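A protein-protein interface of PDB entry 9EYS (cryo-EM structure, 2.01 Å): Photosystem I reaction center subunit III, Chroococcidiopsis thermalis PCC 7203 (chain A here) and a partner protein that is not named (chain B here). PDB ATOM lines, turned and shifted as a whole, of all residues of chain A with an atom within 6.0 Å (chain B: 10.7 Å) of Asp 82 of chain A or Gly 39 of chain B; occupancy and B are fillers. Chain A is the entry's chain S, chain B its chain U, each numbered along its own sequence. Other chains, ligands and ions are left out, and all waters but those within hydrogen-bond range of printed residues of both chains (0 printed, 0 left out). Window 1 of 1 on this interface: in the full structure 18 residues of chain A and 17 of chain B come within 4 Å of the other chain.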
ATOM      1  N   TYR A  61     -12.649  19.084 -10.970  1.00  0.00           N
ATOM      2  CA  TYR A  61     -13.870  18.293 -10.914  1.00  0.00           C
ATOM      3  C   TYR A  61     -13.749  16.989 -10.142  1.00  0.00           C
ATOM      4  O   TYR A  61     -14.772  16.475  -9.681  1.00  0.00           O
ATOM      5  CB  TYR A  61     -14.355  17.973 -12.336  1.00  0.00           C
ATOM      6  CG  TYR A  61     -14.692  19.196 -13.153  1.00  0.00           C
ATOM      7  CD1 TYR A  61     -15.481  20.210 -12.628  1.00  0.00           C
ATOM      8  CD2 TYR A  61     -14.218  19.340 -14.448  1.00  0.00           C
ATOM      9  CE1 TYR A  61     -15.790  21.330 -13.371  1.00  0.00           C
ATOM     10  CE2 TYR A  61     -14.521  20.457 -15.200  1.00  0.00           C
ATOM     11  CZ  TYR A  61     -15.308  21.448 -14.657  1.00  0.00           C
ATOM     12  OH  TYR A  61     -15.612  22.563 -15.403  1.00  0.00           O
ATOM     13  N   GLU A  62     -12.549  16.444  -9.987  1.00  0.00           N
ATOM     14  CA  GLU A  62     -12.381  15.118  -9.415  1.00  0.00           C
ATOM     15  C   GLU A  62     -11.973  15.192  -7.949  1.00  0.00           C
ATOM     16  O   GLU A  62     -11.351  16.159  -7.501  1.00  0.00           O
ATOM     17  CB  GLU A  62     -11.338  14.315 -10.195  1.00  0.00           C
ATOM     18  CG  GLU A  62     -11.688  14.057 -11.655  1.00  0.00           C
ATOM     19  CD  GLU A  62     -12.902  13.162 -11.844  1.00  0.00           C
ATOM     20  OE1 GLU A  62     -13.313  12.977 -13.006  1.00  0.00           O
ATOM     21  OE2 GLU A  62     -13.431  12.625 -10.849  1.00  0.00           O
ATOM     22  N   LEU A  72     -13.693   7.755  -7.723  1.00  0.00           N
ATOM     23  CA  LEU A  72     -15.095   7.988  -8.051  1.00  0.00           C
ATOM     24  C   LEU A  72     -15.976   7.492  -6.915  1.00  0.00           C
ATOM     25  O   LEU A  72     -16.197   6.278  -6.785  1.00  0.00           O
ATOM     26  CB  LEU A  72     -15.463   7.287  -9.362  1.00  0.00           C
ATOM     27  CG  LEU A  72     -14.466   7.464 -10.509  1.00  0.00           C
ATOM     28  CD1 LEU A  72     -14.895   6.661 -11.723  1.00  0.00           C
ATOM     29  CD2 LEU A  72     -14.312   8.933 -10.863  1.00  0.00           C
ATOM     30  N   ARG A  79     -23.086  16.262  -6.940  1.00  0.00           N
ATOM     31  CA  ARG A  79     -22.551  15.641  -8.152  1.00  0.00           C
ATOM     32  C   ARG A  79     -23.291  14.352  -8.498  1.00  0.00           C
ATOM     33  O   ARG A  79     -22.696  13.397  -9.008  1.00  0.00           O
ATOM     34  CB  ARG A  79     -21.036  15.403  -8.028  1.00  0.00           C
ATOM     35  CG  ARG A  79     -20.572  14.335  -7.040  1.00  0.00           C
ATOM     36  CD  ARG A  79     -19.081  14.084  -7.162  1.00  0.00           C
ATOM     37  NE  ARG A  79     -18.305  15.293  -6.917  1.00  0.00           N
ATOM     38  CZ  ARG A  79     -17.028  15.440  -7.241  1.00  0.00           C
ATOM     39  NH1 ARG A  79     -16.348  14.469  -7.829  1.00  0.00           N
ATOM     40  NH2 ARG A  79     -16.418  16.591  -6.972  1.00  0.00           N
ATOM     41  N   ALA A  80     -24.602  14.327  -8.243  1.00  0.00           N
ATOM     42  CA  ALA A  80     -25.409  13.177  -8.634  1.00  0.00           C
ATOM     43  C   ALA A  80     -25.560  13.100 -10.144  1.00  0.00           C
ATOM     44  O   ALA A  80     -25.699  12.005 -10.697  1.00  0.00           O
ATOM     45  CB  ALA A  80     -26.781  13.237  -7.965  1.00  0.00           C
ATOM     46  N   THR A  81     -25.545  14.249 -10.824  1.00  0.00           N
ATOM     47  CA  THR A  81     -25.567  14.242 -12.281  1.00  0.00           C
ATOM     48  C   THR A  81     -24.295  13.632 -12.854  1.00  0.00           C
ATOM     49  O   THR A  81     -24.312  13.100 -13.967  1.00  0.00           O
ATOM     50  CB  THR A  81     -25.763  15.662 -12.812  1.00  0.00           C
ATOM     51  OG1 THR A  81     -24.547  16.403 -12.657  1.00  0.00           O
ATOM     52  CG2 THR A  81     -26.877  16.360 -12.049  1.00  0.00           C
ATOM     53  N   ASP A  82     -23.186  13.698 -12.114  1.00  0.00           N
ATOM     54  CA  ASP A  82     -21.967  13.029 -12.552  1.00  0.00           C
ATOM     55  C   ASP A  82     -22.116  11.515 -12.557  1.00  0.00           C
ATOM     56  O   ASP A  82     -21.357  10.833 -13.253  1.00  0.00           O
ATOM     57  CB  ASP A  82     -20.790  13.437 -11.667  1.00  0.00           C
ATOM     58  CG  ASP A  82     -20.448  14.906 -11.796  1.00  0.00           C
ATOM     59  OD1 ASP A  82     -19.679  15.416 -10.954  1.00  0.00           O
ATOM     60  OD2 ASP A  82     -20.949  15.551 -12.740  1.00  0.00           O
ATOM     61  N   VAL A  83     -23.059  10.980 -11.790  1.00  0.00           N
ATOM     62  CA  VAL A  83     -23.341   9.549 -11.808  1.00  0.00           C
ATOM     63  C   VAL A  83     -24.473   9.221 -12.772  1.00  0.00           C
ATOM     64  O   VAL A  83     -24.401   8.236 -13.510  1.00  0.00           O
ATOM     65  CB  VAL A  83     -23.661   9.061 -10.381  1.00  0.00           C
ATOM     66  CG1 VAL A  83     -23.897   7.560 -10.370  1.00  0.00           C
ATOM     67  CG2 VAL A  83     -22.543   9.440  -9.426  1.00  0.00           C
ATOM     68  N   LEU A  84     -25.523  10.043 -12.789  1.00  0.00           N
ATOM     69  CA  LEU A  84     -26.709   9.728 -13.576  1.00  0.00           C
ATOM     70  C   LEU A  84     -26.511   9.974 -15.066  1.00  0.00           C
ATOM     71  O   LEU A  84     -27.096   9.257 -15.882  1.00  0.00           O
ATOM     72  CB  LEU A  84     -27.905  10.535 -13.069  1.00  0.00           C
ATOM     73  CG  LEU A  84     -28.336  10.251 -11.630  1.00  0.00           C
ATOM     74  CD1 LEU A  84     -29.654  10.941 -11.315  1.00  0.00           C
ATOM     75  CD2 LEU A  84     -28.436   8.752 -11.386  1.00  0.00           C
ATOM     76  N   VAL A  85     -25.722  10.982 -15.444  1.00  0.00           N
ATOM     77  CA  VAL A  85     -25.512  11.257 -16.867  1.00  0.00           C
ATOM     78  C   VAL A  85     -24.795  10.112 -17.575  1.00  0.00           C
ATOM     79  O   VAL A  85     -25.293   9.655 -18.617  1.00  0.00           O
ATOM     80  CB  VAL A  85     -24.803  12.611 -17.047  1.00  0.00           C
ATOM     81  CG1 VAL A  85     -24.231  12.726 -18.447  1.00  0.00           C
ATOM     82  CG2 VAL A  85     -25.769  13.752 -16.774  1.00  0.00           C
ATOM     83  N   PRO A  86     -23.649   9.609 -17.093  1.00  0.00           N
ATOM     84  CA  PRO A  86     -23.042   8.452 -17.776  1.00  0.00           C
ATOM     85  C   PRO A  86     -23.909   7.207 -17.736  1.00  0.00           C
ATOM     86  O   PRO A  86     -23.920   6.434 -18.701  1.00  0.00           O
ATOM     87  CB  PRO A  86     -21.720   8.252 -17.018  1.00  0.00           C
ATOM     88  CG  PRO A  86     -21.464   9.548 -16.338  1.00  0.00           C
ATOM     89  CD  PRO A  86     -22.812  10.060 -15.968  1.00  0.00           C
ATOM     90  N   GLY B  35      -8.821  12.369 -22.482  1.00  0.00           N
ATOM     91  CA  GLY B  35      -8.857  12.388 -21.035  1.00  0.00           C
ATOM     92  C   GLY B  35     -10.222  12.546 -20.406  1.00  0.00           C
ATOM     93  O   GLY B  35     -10.305  12.924 -19.235  1.00  0.00           O
ATOM     94  N   LEU B  36     -11.295  12.275 -21.141  1.00  0.00           N
ATOM     95  CA  LEU B  36     -12.626  12.342 -20.554  1.00  0.00           C
ATOM     96  C   LEU B  36     -12.803  11.235 -19.521  1.00  0.00           C
ATOM     97  O   LEU B  36     -12.412  10.086 -19.744  1.00  0.00           O
ATOM     98  CB  LEU B  36     -13.695  12.238 -21.640  1.00  0.00           C
ATOM     99  CG  LEU B  36     -13.906  13.519 -22.450  1.00  0.00           C
ATOM    100  CD1 LEU B  36     -14.913  13.296 -23.562  1.00  0.00           C
ATOM    101  CD2 LEU B  36     -14.346  14.658 -21.546  1.00  0.00           C
ATOM    102  N   GLN B  37     -13.398  11.588 -18.385  1.00  0.00           N
ATOM    103  CA  GLN B  37     -13.470  10.698 -17.237  1.00  0.00           C
ATOM    104  C   GLN B  37     -14.845  10.834 -16.595  1.00  0.00           C
ATOM    105  O   GLN B  37     -15.551  11.822 -16.804  1.00  0.00           O
ATOM    106  CB  GLN B  37     -12.349  11.022 -16.232  1.00  0.00           C
ATOM    107  CG  GLN B  37     -12.265  10.114 -15.016  1.00  0.00           C
ATOM    108  CD  GLN B  37     -11.977   8.674 -15.384  1.00  0.00           C
ATOM    109  OE1 GLN B  37     -12.863   7.823 -15.345  1.00  0.00           O
ATOM    110  NE2 GLN B  37     -10.730   8.394 -15.741  1.00  0.00           N
ATOM    111  N   TYR B  38     -15.233   9.815 -15.830  1.00  0.00           N
ATOM    112  CA  TYR B  38     -16.465   9.895 -15.057  1.00  0.00           C
ATOM    113  C   TYR B  38     -16.379  11.047 -14.064  1.00  0.00           C
ATOM    114  O   TYR B  38     -15.390  11.185 -13.340  1.00  0.00           O
ATOM    115  CB  TYR B  38     -16.724   8.578 -14.328  1.00  0.00           C
ATOM    116  CG  TYR B  38     -17.134   7.447 -15.242  1.00  0.00           C
ATOM    117  CD1 TYR B  38     -18.469   7.219 -15.540  1.00  0.00           C
ATOM    118  CD2 TYR B  38     -16.184   6.605 -15.803  1.00  0.00           C
ATOM    119  CE1 TYR B  38     -18.847   6.187 -16.375  1.00  0.00           C
ATOM    120  CE2 TYR B  38     -16.553   5.571 -16.639  1.00  0.00           C
ATOM    121  CZ  TYR B  38     -17.886   5.367 -16.921  1.00  0.00           C
ATOM    122  OH  TYR B  38     -18.261   4.339 -17.752  1.00  0.00           O
ATOM    123  N   GLY B  39     -17.424  11.868 -14.027  1.00  0.00           N
ATOM    124  CA  GLY B  39     -17.387  13.110 -13.289  1.00  0.00           C
ATOM    125  C   GLY B  39     -16.786  14.272 -14.047  1.00  0.00           C
ATOM    126  O   GLY B  39     -16.558  15.330 -13.447  1.00  0.00           O
ATOM    127  N   THR B  40     -16.513  14.106 -15.341  1.00  0.00           N
ATOM    128  CA  THR B  40     -15.928  15.154 -16.162  1.00  0.00           C
ATOM    129  C   THR B  40     -16.688  15.388 -17.463  1.00  0.00           C
ATOM    130  O   THR B  40     -16.589  16.485 -18.023  1.00  0.00           O
ATOM    131  CB  THR B  40     -14.455  14.819 -16.471  1.00  0.00           C
ATOM    132  OG1 THR B  40     -13.728  14.713 -15.241  1.00  0.00           O
ATOM    133  CG2 THR B  40     -13.792  15.892 -17.323  1.00  0.00           C
ATOM    134  N   TYR B  41     -17.480  14.421 -17.929  1.00  0.00           N
ATOM    135  CA  TYR B  41     -18.176  14.564 -19.202  1.00  0.00           C
ATOM    136  C   TYR B  41     -19.093  15.779 -19.193  1.00  0.00           C
ATOM    137  O   TYR B  41     -19.736  16.087 -18.186  1.00  0.00           O
ATOM    138  CB  TYR B  41     -19.004  13.318 -19.516  1.00  0.00           C
ATOM    139  CG  TYR B  41     -18.266  12.007 -19.424  1.00  0.00           C
ATOM    140  CD1 TYR B  41     -18.459  11.159 -18.345  1.00  0.00           C
ATOM    141  CD2 TYR B  41     -17.386  11.610 -20.420  1.00  0.00           C
ATOM    142  CE1 TYR B  41     -17.798   9.956 -18.259  1.00  0.00           C
ATOM    143  CE2 TYR B  41     -16.716  10.409 -20.339  1.00  0.00           C
ATOM    144  CZ  TYR B  41     -16.925   9.587 -19.255  1.00  0.00           C
ATOM    145  OH  TYR B  41     -16.264   8.388 -19.166  1.00  0.00           O
ATOM    146  N   PHE B  42     -19.145  16.468 -20.334  1.00  0.00           N
ATOM    147  CA  PHE B  42     -20.059  17.588 -20.550  1.00  0.00           C
ATOM    148  C   PHE B  42     -19.842  18.709 -19.539  1.00  0.00           C
ATOM    149  O   PHE B  42     -20.793  19.366 -19.107  1.00  0.00           O
ATOM    150  CB  PHE B  42     -21.516  17.118 -20.535  1.00  0.00           C
ATOM    151  CG  PHE B  42     -21.750  15.860 -21.322  1.00  0.00           C
ATOM    152  CD1 PHE B  42     -21.292  15.747 -22.623  1.00  0.00           C
ATOM    153  CD2 PHE B  42     -22.419  14.788 -20.758  1.00  0.00           C
ATOM    154  CE1 PHE B  42     -21.503  14.592 -23.350  1.00  0.00           C
ATOM    155  CE2 PHE B  42     -22.632  13.629 -21.481  1.00  0.00           C
ATOM    156  CZ  PHE B  42     -22.174  13.531 -22.777  1.00  0.00           C
ATOM    157  N   LYS B  43     -18.588  18.936 -19.155  1.00  0.00           N
ATOM    158  CA  LYS B  43     -18.230  20.069 -18.326  1.00  0.00           C
ATOM    159  C   LYS B  43     -17.236  20.959 -19.059  1.00  0.00           C
ATOM    160  O   LYS B  43     -16.370  20.454 -19.781  1.00  0.00           O
ATOM    161  CB  LYS B  43     -17.628  19.619 -16.987  1.00  0.00           C
ATOM    162  CG  LYS B  43     -18.617  18.926 -16.071  1.00  0.00           C
ATOM    163  CD  LYS B  43     -17.969  18.537 -14.757  1.00  0.00           C
ATOM    164  CE  LYS B  43     -18.954  17.826 -13.850  1.00  0.00           C
ATOM    165  NZ  LYS B  43     -18.328  17.429 -12.561  1.00  0.00           N
ATOM    166  N   PRO B  44     -17.337  22.277 -18.905  1.00  0.00           N
ATOM    167  CA  PRO B  44     -16.459  23.178 -19.659  1.00  0.00           C
ATOM    168  C   PRO B  44     -15.003  23.029 -19.253  1.00  0.00           C
ATOM    169  O   PRO B  44     -14.679  22.678 -18.116  1.00  0.00           O
ATOM    170  CB  PRO B  44     -16.996  24.570 -19.310  1.00  0.00           C
ATOM    171  CG  PRO B  44     -17.653  24.393 -17.984  1.00  0.00           C
ATOM    172  CD  PRO B  44     -18.238  23.012 -17.999  1.00  0.00           C
ATOM    173  N   PRO B  46     -11.550  24.047 -17.928  1.00  0.00           N
ATOM    174  CA  PRO B  46     -11.065  25.086 -17.014  1.00  0.00           C
ATOM    175  C   PRO B  46      -9.923  25.901 -17.612  1.00  0.00           C
ATOM    176  O   PRO B  46      -9.805  27.102 -17.366  1.00  0.00           O
ATOM    177  CB  PRO B  46     -10.586  24.285 -15.803  1.00  0.00           C
ATOM    178  CG  PRO B  46     -10.216  22.956 -16.356  1.00  0.00           C
ATOM    179  CD  PRO B  46     -11.177  22.694 -17.480  1.00  0.00           C
ATOM    180  OXT PRO B  46      -9.093  25.380 -18.356  1.00  0.00           O
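The backbone carbonyl oxygen (O) of Pro 44 of chain B sits at hydrogen-bond distance from the side-chain hydroxyl (OH) of Tyr 61 of chain A, at 2.9 Å.
The side-chain carboxylate of Glu 62 of chain A is in hydrogen-bond range of the side-chain hydroxyl of Thr 40 of chain B (2.9 Å).
The side-chain amino group (NZ) of Lys 43 of chain B lies within salt-bridge range of the side-chain carboxylate (OD1) of Asp 82 of chain A (2.9 Å).
O of Tyr 38 of chain B lies close to OE1 of Glu 62 of chain A.
O of Tyr 61 of chain A lies within hydrogen-bond range of NH1 of Arg 79 of chain A.
The backbone carbonyl oxygen (O) of Gly 39 of chain B sits at hydrogen-bond distance from the side-chain amino group (NZ) of Lys 43 of chain B (2.9 Å).
Among the printed residues, pairs that only touch across the chains: Tyr 61 of chain A with Gly 39 of chain B, Tyr 61 of chain A with Lys 43 of chain B, Glu 62 of chain A with Gln 37 of chain B, Glu 62 of chain A with Gly 39 of chain B, Leu 72 of chain A with Tyr 38 of chain B, Asp 82 of chain A with Gly 39 of chain B, Val 85 of chain A with Phe 42 of chain B, Pro 86 of chain A with Tyr 38 of chain B and Pro 86 of chain A with Tyr 41 of chain B.
Of the 11 printed residues of chain B, 8 touch a printed residue of chain A.
Hydrophobic or aromatic side chains of chain B that line the printed part of chain A: Tyr 38, Tyr 41, Phe 42 and Pro 44.
Among the printed residues, 13 pairs touch across the chains.
Among the printed residues, Asp or Glu carboxylates within 4 Å of a Lys or Arg side-chain nitrogen of the other chain: Asp 82 of chain A with Lys 43 of chain B (2.9 Å).
Of the printed residues of chain B, Asp 82 of chain A touches Gly 39 and Lys 43.
Gly 39 of chain B touches three residues of chain A.
No residue of chain B comes within 4 Å of Val 83 of chain A.
Printed residues of chain B within 4 Å of Glu 62 of chain A: Gln 37 (3.7 Å), Tyr 38 (2.8 Å), Gly 39 (3.8 Å) and Thr 40 (2.9 Å).
Printed residues of chain A within 4 Å of Lys 43 of chain B: Tyr 61 (3.7 Å) and Asp 82 (2.9 Å).
The nearest residue of chain A that does not touch Gly 39 of chain B is Pro 86 of chain A (5.2 Å).
The nearest printed residue of chain B that does not touch Tyr 61 of chain A is Thr 40 of chain B (4.4 Å).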
